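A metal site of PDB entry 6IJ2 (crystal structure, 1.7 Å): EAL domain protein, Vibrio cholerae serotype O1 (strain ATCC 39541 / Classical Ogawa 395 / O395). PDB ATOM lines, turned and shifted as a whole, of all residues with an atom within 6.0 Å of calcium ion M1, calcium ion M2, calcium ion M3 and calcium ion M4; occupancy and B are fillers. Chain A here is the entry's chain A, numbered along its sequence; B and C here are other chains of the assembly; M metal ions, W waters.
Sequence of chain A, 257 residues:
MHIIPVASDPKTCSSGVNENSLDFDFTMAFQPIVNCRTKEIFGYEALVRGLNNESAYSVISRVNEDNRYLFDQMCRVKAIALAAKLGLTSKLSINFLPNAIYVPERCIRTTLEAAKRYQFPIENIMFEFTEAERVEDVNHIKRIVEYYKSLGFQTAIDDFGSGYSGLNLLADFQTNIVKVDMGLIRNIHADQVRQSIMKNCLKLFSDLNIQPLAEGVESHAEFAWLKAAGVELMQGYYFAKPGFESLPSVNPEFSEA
OD1 of Asn 95 lies close to O2' of G 2 of chain B (3.4 Å). The side-chain carboxylate of Glu 215 sits close to the side-chain amino group of Lys 179, at 3.5 Å. N of Glu 215 lies within hydrogen-bond range of O of Val 180 (3.0 Å). The side-chain carboxylate of Glu 128 is in salt-bridge range of the side-chain amino group of Lys 179 (2.8 Å). OG of Ser 162 is in hydrogen-bond range of OD1 of Asp 181 (3.2 Å). OE1 of Glu 45 lies within salt-bridge range of NZ of Lys 179 (3.3 Å).
Within 4 Å of calcium ion M1: Asp 158, Asp 159, Glu 215 and G 1 of chain B. Along chain A the residues within 4 Å of calcium ion M1 span positions 158 to 215. The nearest printed residue that does not touch calcium ion M1 is Lys 179 (4.7 Å).
Within 4 Å of calcium ion M2: Glu 45, Asn 95, Glu 128, Asp 158 and G 1 of chain B.
Of the 23 residues printed, 3 come within 4 Å of calcium ion M3.
Within 4 Å of calcium ion M4: Thr 130, Asp 158, Asp 159 and G 1 of chain B.
Calcium ion M1 is bound by water W5. The side-chain carboxylate (OD1) of Asp 158 is bound to calcium ion M1. OP3 of G 1 of chain B is bound to calcium ion M1, at 2.3 Å. Calcium ion M1 is bound by OE2 of Glu 215, 2.3 Å away. The backbone carbonyl oxygen (O) of Asp 158 binds calcium ion M1, at 2.4 Å. OD1 of Asp 159 is bound to calcium ion M1, at 2.4 Å. Calcium ion M1 is bound by OE1 of Glu 215 (2.5 Å).
Calcium ion M2 is bound by OE2 of Glu 128 (2.3 Å), water W1 (2.3 Å), OD1 of Asn 95 (2.4 Å), OE2 of Glu 45 (2.4 Å), OD2 of Asp 158 (2.4 Å), OP1 of G 1 of chain B (2.4 Å) and OD1 of Asp 158 (2.7 Å). Calcium ion M2 has seven donor atoms within binding distance.
Calcium ion M3 is bound by O of Ser 162 (2.2 Å). O of Tyr 164 binds calcium ion M3 (2.2 Å). Water W2 is bound to calcium ion M3, 2.4 Å away. O of Asp 159 binds calcium ion M3, 2.4 Å away. Calcium ion M3 is bound by water W4, 2.5 Å away. Calcium ion M3 has five donor atoms within binding distance.
Water W3 binds calcium ion M4 (2.4 Å). The side-chain carboxylate (OD2) of Asp 159 is bound to calcium ion M4 (2.5 Å). OP2 of G 1 of chain B is bound to calcium ion M4 (2.7 Å). Calcium ion M4 is bound by the side-chain hydroxyl (OG1) of Thr 130 (2.8 Å). OD1 of Asp 159 is bound to calcium ion M4 (2.8 Å).
Water W1 lies within hydrogen-bond range of OE1 of Glu 45 and NZ of Lys 179. Water W4 lies within hydrogen-bond range of the side-chain carboxylate of Glu 131 and the backbone NH of Tyr 164.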
ATOM      1  N   GLU A  45      27.434  -2.453  22.766  1.00  0.00           N
ATOM      2  CA  GLU A  45      27.933  -2.499  21.411  1.00  0.00           C
ATOM      3  C   GLU A  45      27.859  -1.092  20.816  1.00  0.00           C
ATOM      4  O   GLU A  45      26.827  -0.411  20.951  1.00  0.00           O
ATOM      5  CB  GLU A  45      27.141  -3.484  20.552  1.00  0.00           C
ATOM      6  CG  GLU A  45      27.645  -3.518  19.133  1.00  0.00           C
ATOM      7  CD  GLU A  45      26.892  -4.470  18.232  1.00  0.00           C
ATOM      8  OE1 GLU A  45      25.830  -5.005  18.632  1.00  0.00           O
ATOM      9  OE2 GLU A  45      27.396  -4.671  17.105  1.00  0.00           O
ATOM     10  N   LEU A  47      27.641   1.352  17.660  1.00  0.00           N
ATOM     11  CA  LEU A  47      26.989   1.251  16.357  1.00  0.00           C
ATOM     12  C   LEU A  47      27.060   2.598  15.660  1.00  0.00           C
ATOM     13  O   LEU A  47      26.687   3.619  16.248  1.00  0.00           O
ATOM     14  CB  LEU A  47      25.536   0.822  16.503  1.00  0.00           C
ATOM     15  CG  LEU A  47      25.342  -0.559  17.136  1.00  0.00           C
ATOM     16  CD1 LEU A  47      23.924  -0.667  17.638  1.00  0.00           C
ATOM     17  CD2 LEU A  47      25.635  -1.660  16.114  1.00  0.00           C
ATOM     18  N   ASN A  95      32.400  -3.335  16.192  1.00  0.00           N
ATOM     19  CA  ASN A  95      32.265  -4.159  14.994  1.00  0.00           C
ATOM     20  C   ASN A  95      33.516  -4.001  14.135  1.00  0.00           C
ATOM     21  O   ASN A  95      33.939  -2.881  13.837  1.00  0.00           O
ATOM     22  CB  ASN A  95      31.033  -3.737  14.195  1.00  0.00           C
ATOM     23  CG  ASN A  95      29.741  -4.138  14.867  1.00  0.00           C
ATOM     24  OD1 ASN A  95      29.325  -5.290  14.814  1.00  0.00           O
ATOM     25  ND2 ASN A  95      29.092  -3.175  15.517  1.00  0.00           N
ATOM     26  N   GLU A 128      33.980  -7.583  17.453  1.00  0.00           N
ATOM     27  CA  GLU A 128      33.040  -8.522  16.852  1.00  0.00           C
ATOM     28  C   GLU A 128      33.410  -8.734  15.387  1.00  0.00           C
ATOM     29  O   GLU A 128      33.546  -7.764  14.631  1.00  0.00           O
ATOM     30  CB  GLU A 128      31.606  -8.016  16.968  1.00  0.00           C
ATOM     31  CG  GLU A 128      31.250  -7.620  18.386  1.00  0.00           C
ATOM     32  CD  GLU A 128      29.797  -7.256  18.548  1.00  0.00           C
ATOM     33  OE1 GLU A 128      29.394  -6.977  19.690  1.00  0.00           O
ATOM     34  OE2 GLU A 128      29.044  -7.265  17.541  1.00  0.00           O
ATOM     35  N   THR A 130      32.890 -10.225  11.632  1.00  0.00           N
ATOM     36  CA  THR A 130      32.030 -10.650  10.542  1.00  0.00           C
ATOM     37  C   THR A 130      32.905 -10.891   9.315  1.00  0.00           C
ATOM     38  O   THR A 130      33.806 -10.096   9.010  1.00  0.00           O
ATOM     39  CB  THR A 130      30.966  -9.593  10.194  1.00  0.00           C
ATOM     40  OG1 THR A 130      30.160  -9.313  11.347  1.00  0.00           O
ATOM     41  CG2 THR A 130      30.069 -10.093   9.068  1.00  0.00           C
ATOM     42  N   GLU A 131      32.630 -11.980   8.611  1.00  0.00           N
ATOM     43  CA  GLU A 131      33.382 -12.317   7.405  1.00  0.00           C
ATOM     44  C   GLU A 131      32.998 -11.397   6.251  1.00  0.00           C
ATOM     45  O   GLU A 131      31.846 -10.965   6.134  1.00  0.00           O
ATOM     46  CB  GLU A 131      33.129 -13.770   7.022  1.00  0.00           C
ATOM     47  CG  GLU A 131      33.248 -14.756   8.187  1.00  0.00           C
ATOM     48  CD  GLU A 131      31.915 -15.027   8.888  1.00  0.00           C
ATOM     49  OE1 GLU A 131      31.211 -14.049   9.224  1.00  0.00           O
ATOM     50  OE2 GLU A 131      31.579 -16.214   9.088  1.00  0.00           O
ATOM     51  N   ILE A 157      32.538 -13.895  17.604  1.00  0.00           N
ATOM     52  CA  ILE A 157      31.929 -14.130  16.300  1.00  0.00           C
ATOM     53  C   ILE A 157      30.572 -13.444  16.303  1.00  0.00           C
ATOM     54  O   ILE A 157      29.722 -13.711  17.149  1.00  0.00           O
ATOM     55  CB  ILE A 157      31.808 -15.639  16.003  1.00  0.00           C
ATOM     56  CG1 ILE A 157      33.200 -16.242  15.871  1.00  0.00           C
ATOM     57  CG2 ILE A 157      30.990 -15.865  14.735  1.00  0.00           C
ATOM     58  CD1 ILE A 157      33.196 -17.709  15.648  1.00  0.00           C
ATOM     59  N   ASP A 158      30.377 -12.516  15.360  1.00  0.00           N
ATOM     60  CA  ASP A 158      29.201 -11.641  15.393  1.00  0.00           C
ATOM     61  C   ASP A 158      27.937 -12.343  14.886  1.00  0.00           C
ATOM     62  O   ASP A 158      26.848 -12.180  15.450  1.00  0.00           O
ATOM     63  CB  ASP A 158      29.513 -10.399  14.557  1.00  0.00           C
ATOM     64  CG  ASP A 158      28.567  -9.232  14.800  1.00  0.00           C
ATOM     65  OD1 ASP A 158      27.554  -9.371  15.522  1.00  0.00           O
ATOM     66  OD2 ASP A 158      28.865  -8.145  14.281  1.00  0.00           O
ATOM     67  N   ASP A 159      28.041 -13.121  13.836  1.00  0.00           N
ATOM     68  CA  ASP A 159      26.819 -13.451  13.118  1.00  0.00           C
ATOM     69  C   ASP A 159      26.669 -14.952  13.027  1.00  0.00           C
ATOM     70  O   ASP A 159      26.481 -15.494  11.938  1.00  0.00           O
ATOM     71  CB  ASP A 159      26.804 -12.819  11.729  1.00  0.00           C
ATOM     72  CG  ASP A 159      26.968 -11.288  11.766  1.00  0.00           C
ATOM     73  OD1 ASP A 159      26.770 -10.664  12.826  1.00  0.00           O
ATOM     74  OD2 ASP A 159      27.276 -10.708  10.688  1.00  0.00           O
ATOM     75  N   PHE A 160      26.735 -15.650  14.151  1.00  0.00           N
ATOM     76  CA  PHE A 160      26.518 -17.097  14.117  1.00  0.00           C
ATOM     77  C   PHE A 160      25.059 -17.409  13.785  1.00  0.00           C
ATOM     78  O   PHE A 160      24.138 -16.957  14.457  1.00  0.00           O
ATOM     79  CB  PHE A 160      26.882 -17.732  15.441  1.00  0.00           C
ATOM     80  CG  PHE A 160      26.853 -19.229  15.410  1.00  0.00           C
ATOM     81  CD1 PHE A 160      27.977 -19.943  15.046  1.00  0.00           C
ATOM     82  CD2 PHE A 160      25.707 -19.915  15.747  1.00  0.00           C
ATOM     83  CE1 PHE A 160      27.964 -21.324  15.029  1.00  0.00           C
ATOM     84  CE2 PHE A 160      25.669 -21.300  15.718  1.00  0.00           C
ATOM     85  CZ  PHE A 160      26.802 -21.995  15.363  1.00  0.00           C
ATOM     86  N   GLY A 161      24.857 -18.230  12.774  1.00  0.00           N
ATOM     87  CA  GLY A 161      23.520 -18.587  12.365  1.00  0.00           C
ATOM     88  C   GLY A 161      22.941 -17.756  11.248  1.00  0.00           C
ATOM     89  O   GLY A 161      21.758 -17.932  10.928  1.00  0.00           O
ATOM     90  N   SER A 162      23.721 -16.874  10.644  1.00  0.00           N
ATOM     91  CA  SER A 162      23.304 -16.174   9.442  1.00  0.00           C
ATOM     92  C   SER A 162      24.515 -15.919   8.557  1.00  0.00           C
ATOM     93  O   SER A 162      25.651 -16.155   8.961  1.00  0.00           O
ATOM     94  CB  SER A 162      22.625 -14.844   9.773  1.00  0.00           C
ATOM     95  OG  SER A 162      23.569 -13.966  10.351  1.00  0.00           O
ATOM     96  N   GLY A 163      24.276 -15.426   7.358  1.00  0.00           N
ATOM     97  CA  GLY A 163      25.389 -15.025   6.518  1.00  0.00           C
ATOM     98  C   GLY A 163      26.308 -16.184   6.150  1.00  0.00           C
ATOM     99  O   GLY A 163      25.867 -17.191   5.568  1.00  0.00           O
ATOM    100  N   TYR A 164      27.583 -16.057   6.490  1.00  0.00           N
ATOM    101  CA  TYR A 164      28.586 -17.075   6.218  1.00  0.00           C
ATOM    102  C   TYR A 164      28.626 -18.101   7.342  1.00  0.00           C
ATOM    103  O   TYR A 164      28.145 -17.862   8.443  1.00  0.00           O
ATOM    104  CB  TYR A 164      29.941 -16.406   6.007  1.00  0.00           C
ATOM    105  CG  TYR A 164      29.893 -15.433   4.834  1.00  0.00           C
ATOM    106  CD1 TYR A 164      29.834 -15.903   3.541  1.00  0.00           C
ATOM    107  CD2 TYR A 164      29.869 -14.054   5.041  1.00  0.00           C
ATOM    108  CE1 TYR A 164      29.778 -15.036   2.461  1.00  0.00           C
ATOM    109  CE2 TYR A 164      29.819 -13.175   3.962  1.00  0.00           C
ATOM    110  CZ  TYR A 164      29.761 -13.668   2.673  1.00  0.00           C
ATOM    111  OH  TYR A 164      29.713 -12.813   1.598  1.00  0.00           O
ATOM    112  N   SER A 165      29.202 -19.275   7.050  1.00  0.00           N
ATOM    113  CA  SER A 165      29.150 -20.399   7.983  1.00  0.00           C
ATOM    114  C   SER A 165      29.981 -20.106   9.223  1.00  0.00           C
ATOM    115  O   SER A 165      31.211 -20.004   9.141  1.00  0.00           O
ATOM    116  CB  SER A 165      29.641 -21.685   7.311  1.00  0.00           C
ATOM    117  OG  SER A 165      29.772 -22.728   8.287  1.00  0.00           O
ATOM    118  N   GLY A 166      29.304 -19.988  10.370  1.00  0.00           N
ATOM    119  CA  GLY A 166      30.009 -19.821  11.627  1.00  0.00           C
ATOM    120  C   GLY A 166      30.681 -21.085  12.109  1.00  0.00           C
ATOM    121  O   GLY A 166      31.705 -21.029  12.773  1.00  0.00           O
ATOM    122  N   LYS A 179      28.098 -14.559  19.235  1.00  0.00           N
ATOM    123  CA  LYS A 179      26.806 -13.891  19.207  1.00  0.00           C
ATOM    124  C   LYS A 179      25.887 -14.643  18.250  1.00  0.00           C
ATOM    125  O   LYS A 179      26.265 -14.904  17.107  1.00  0.00           O
ATOM    126  CB  LYS A 179      26.950 -12.436  18.755  1.00  0.00           C
ATOM    127  CG  LYS A 179      27.827 -11.659  19.727  1.00  0.00           C
ATOM    128  CD  LYS A 179      27.170 -10.361  20.217  1.00  0.00           C
ATOM    129  CE  LYS A 179      27.295  -9.281  19.241  1.00  0.00           C
ATOM    130  NZ  LYS A 179      26.746  -7.960  19.731  1.00  0.00           N
ATOM    131  N   VAL A 180      24.693 -14.989  18.719  1.00  0.00           N
ATOM    132  CA  VAL A 180      23.765 -15.800  17.926  1.00  0.00           C
ATOM    133  C   VAL A 180      22.783 -14.871  17.251  1.00  0.00           C
ATOM    134  O   VAL A 180      22.064 -14.110  17.910  1.00  0.00           O
ATOM    135  CB  VAL A 180      23.037 -16.845  18.796  1.00  0.00           C
ATOM    136  CG1 VAL A 180      22.045 -17.644  17.919  1.00  0.00           C
ATOM    137  CG2 VAL A 180      24.045 -17.774  19.433  1.00  0.00           C
ATOM    138  N   ASP A 181      22.711 -14.983  15.915  1.00  0.00           N
ATOM    139  CA  ASP A 181      21.897 -14.097  15.102  1.00  0.00           C
ATOM    140  C   ASP A 181      20.437 -14.150  15.544  1.00  0.00           C
ATOM    141  O   ASP A 181      19.922 -15.200  15.911  1.00  0.00           O
ATOM    142  CB  ASP A 181      22.015 -14.495  13.636  1.00  0.00           C
ATOM    143  CG  ASP A 181      21.218 -13.584  12.731  1.00  0.00           C
ATOM    144  OD1 ASP A 181      21.674 -12.458  12.481  1.00  0.00           O
ATOM    145  OD2 ASP A 181      20.137 -13.990  12.268  1.00  0.00           O
ATOM    146  N   GLU A 215      21.386 -12.406  20.316  1.00  0.00           N
ATOM    147  CA  GLU A 215      21.102 -11.122  19.683  1.00  0.00           C
ATOM    148  C   GLU A 215      19.626 -10.962  19.331  1.00  0.00           C
ATOM    149  O   GLU A 215      18.928 -11.932  19.025  1.00  0.00           O
ATOM    150  CB  GLU A 215      21.918 -10.932  18.406  1.00  0.00           C
ATOM    151  CG  GLU A 215      23.431 -10.928  18.568  1.00  0.00           C
ATOM    152  CD  GLU A 215      24.153 -10.633  17.258  1.00  0.00           C
ATOM    153  OE1 GLU A 215      25.119  -9.859  17.281  1.00  0.00           O
ATOM    154  OE2 GLU A 215      23.757 -11.157  16.186  1.00  0.00           O
ATOM    155  OP3   G B   1      24.719  -8.163  14.292  1.00  0.00           O
ATOM    156  P     G B   1      24.956  -6.952  13.552  1.00  0.00           P
ATOM    157  OP1   G B   1      25.992  -6.177  14.149  1.00  0.00           O
ATOM    158  OP2   G B   1      25.141  -7.366  12.199  1.00  0.00           O
ATOM    159  O5'   G B   1      23.568  -6.215  13.637  1.00  0.00           O
ATOM    160  C5'   G B   1      23.379  -5.089  14.486  1.00  0.00           C
ATOM    161  C4'   G B   1      22.089  -4.389  14.119  1.00  0.00           C
ATOM    162  O4'   G B   1      20.988  -5.019  14.804  1.00  0.00           O
ATOM    163  C3'   G B   1      21.990  -2.908  14.484  1.00  0.00           C
ATOM    164  O3'   G B   1      21.521  -2.099  13.424  1.00  0.00           O
ATOM    165  C2'   G B   1      20.967  -2.880  15.604  1.00  0.00           C
ATOM    166  O2'   G B   1      20.153  -1.745  15.664  1.00  0.00           O
ATOM    167  C1'   G B   1      20.083  -4.056  15.216  1.00  0.00           C
ATOM    168  N9    G B   1      19.313  -4.582  16.334  1.00  0.00           N
ATOM    169  C8    G B   1      19.720  -4.657  17.652  1.00  0.00           C
ATOM    170  N7    G B   1      18.824  -5.197  18.429  1.00  0.00           N
ATOM    171  C5    G B   1      17.776  -5.504  17.575  1.00  0.00           C
ATOM    172  C6    G B   1      16.523  -6.107  17.849  1.00  0.00           C
ATOM    173  O6    G B   1      16.074  -6.495  18.918  1.00  0.00           O
ATOM    174  N1    G B   1      15.748  -6.224  16.707  1.00  0.00           N
ATOM    175  C2    G B   1      16.142  -5.818  15.453  1.00  0.00           C
ATOM    176  N2    G B   1      15.271  -6.041  14.470  1.00  0.00           N
ATOM    177  N3    G B   1      17.307  -5.270  15.180  1.00  0.00           N
ATOM    178  C4    G B   1      18.069  -5.143  16.282  1.00  0.00           C
ATOM    179  P     G B   2      22.315  -0.889  12.957  1.00  0.00           P
ATOM    180  OP1   G B   2      22.807  -0.221  14.119  1.00  0.00           O
ATOM    181  OP2   G B   2      21.485  -0.186  12.034  1.00  0.00           O
ATOM    182  O5'   G B   2      23.517  -1.509  12.147  1.00  0.00           O
ATOM    183  C5'   G B   2      23.358  -1.963  10.809  1.00  0.00           C
ATOM    184  C4'   G B   2      24.609  -2.685  10.367  1.00  0.00           C
ATOM    185  O4'   G B   2      25.734  -1.792  10.469  1.00  0.00           O
ATOM    186  C3'   G B   2      24.975  -3.921  11.192  1.00  0.00           C
ATOM    187  O3'   G B   2      25.398  -4.995  10.369  1.00  0.00           O
ATOM    188  C2'   G B   2      26.180  -3.454  12.002  1.00  0.00           C
ATOM    189  O2'   G B   2      27.104  -4.450  12.344  1.00  0.00           O
ATOM    190  C1'   G B   2      26.808  -2.458  11.042  1.00  0.00           C
ATOM    191  N9    G B   2      27.617  -1.491  11.775  1.00  0.00           N
ATOM    192  C8    G B   2      27.179  -0.606  12.716  1.00  0.00           C
ATOM    193  N7    G B   2      28.137   0.084  13.252  1.00  0.00           N
ATOM    194  C5    G B   2      29.286  -0.393  12.639  1.00  0.00           C
ATOM    195  C6    G B   2      30.633  -0.026  12.810  1.00  0.00           C
ATOM    196  O6    G B   2      31.116   0.798  13.585  1.00  0.00           O
ATOM    197  N1    G B   2      31.469  -0.759  11.986  1.00  0.00           N
ATOM    198  C2    G B   2      31.063  -1.730  11.111  1.00  0.00           C
ATOM    199  N2    G B   2      32.018  -2.324  10.408  1.00  0.00           N
ATOM    200  N3    G B   2      29.804  -2.064  10.928  1.00  0.00           N
ATOM    201  C4    G B   2      28.973  -1.361  11.719  1.00  0.00           C
ATOM    202  N   SER C 165      25.867 -20.011   5.774  1.00  0.00           N
ATOM    203  CA  SER C 165      25.417 -20.632   7.026  1.00  0.00           C
ATOM    204  C   SER C 165      24.365 -21.710   6.762  1.00  0.00           C
ATOM    205  O   SER C 165      23.254 -21.405   6.336  1.00  0.00           O
ATOM    206  CB  SER C 165      24.870 -19.563   7.975  1.00  0.00           C
ATOM    207  OG  SER C 165      24.219 -20.150   9.108  1.00  0.00           O
HETATM  208 CA    CA M   1      25.503 -10.289  14.887  1.00  0.00          CA
HETATM  209 CA    CA M   2      27.686  -6.685  15.815  1.00  0.00          CA
HETATM  210 CA    CA M   3      27.634 -16.315   9.964  1.00  0.00          CA
HETATM  211 CA    CA M   4      27.544  -8.369  11.421  1.00  0.00          CA
HETATM  212  O   HOH W   1      25.764  -7.200  17.016  1.00  0.00           O
HETATM  213  O   HOH W   2      29.689 -16.432  11.166  1.00  0.00           O
HETATM  214  O   HOH W   3      28.172  -6.434  10.161  1.00  0.00           O
HETATM  215  O   HOH W   4      28.534 -14.335   8.718  1.00  0.00           O
HETATM  216  O   HOH W   5      24.204 -11.259  13.207  1.00  0.00           O
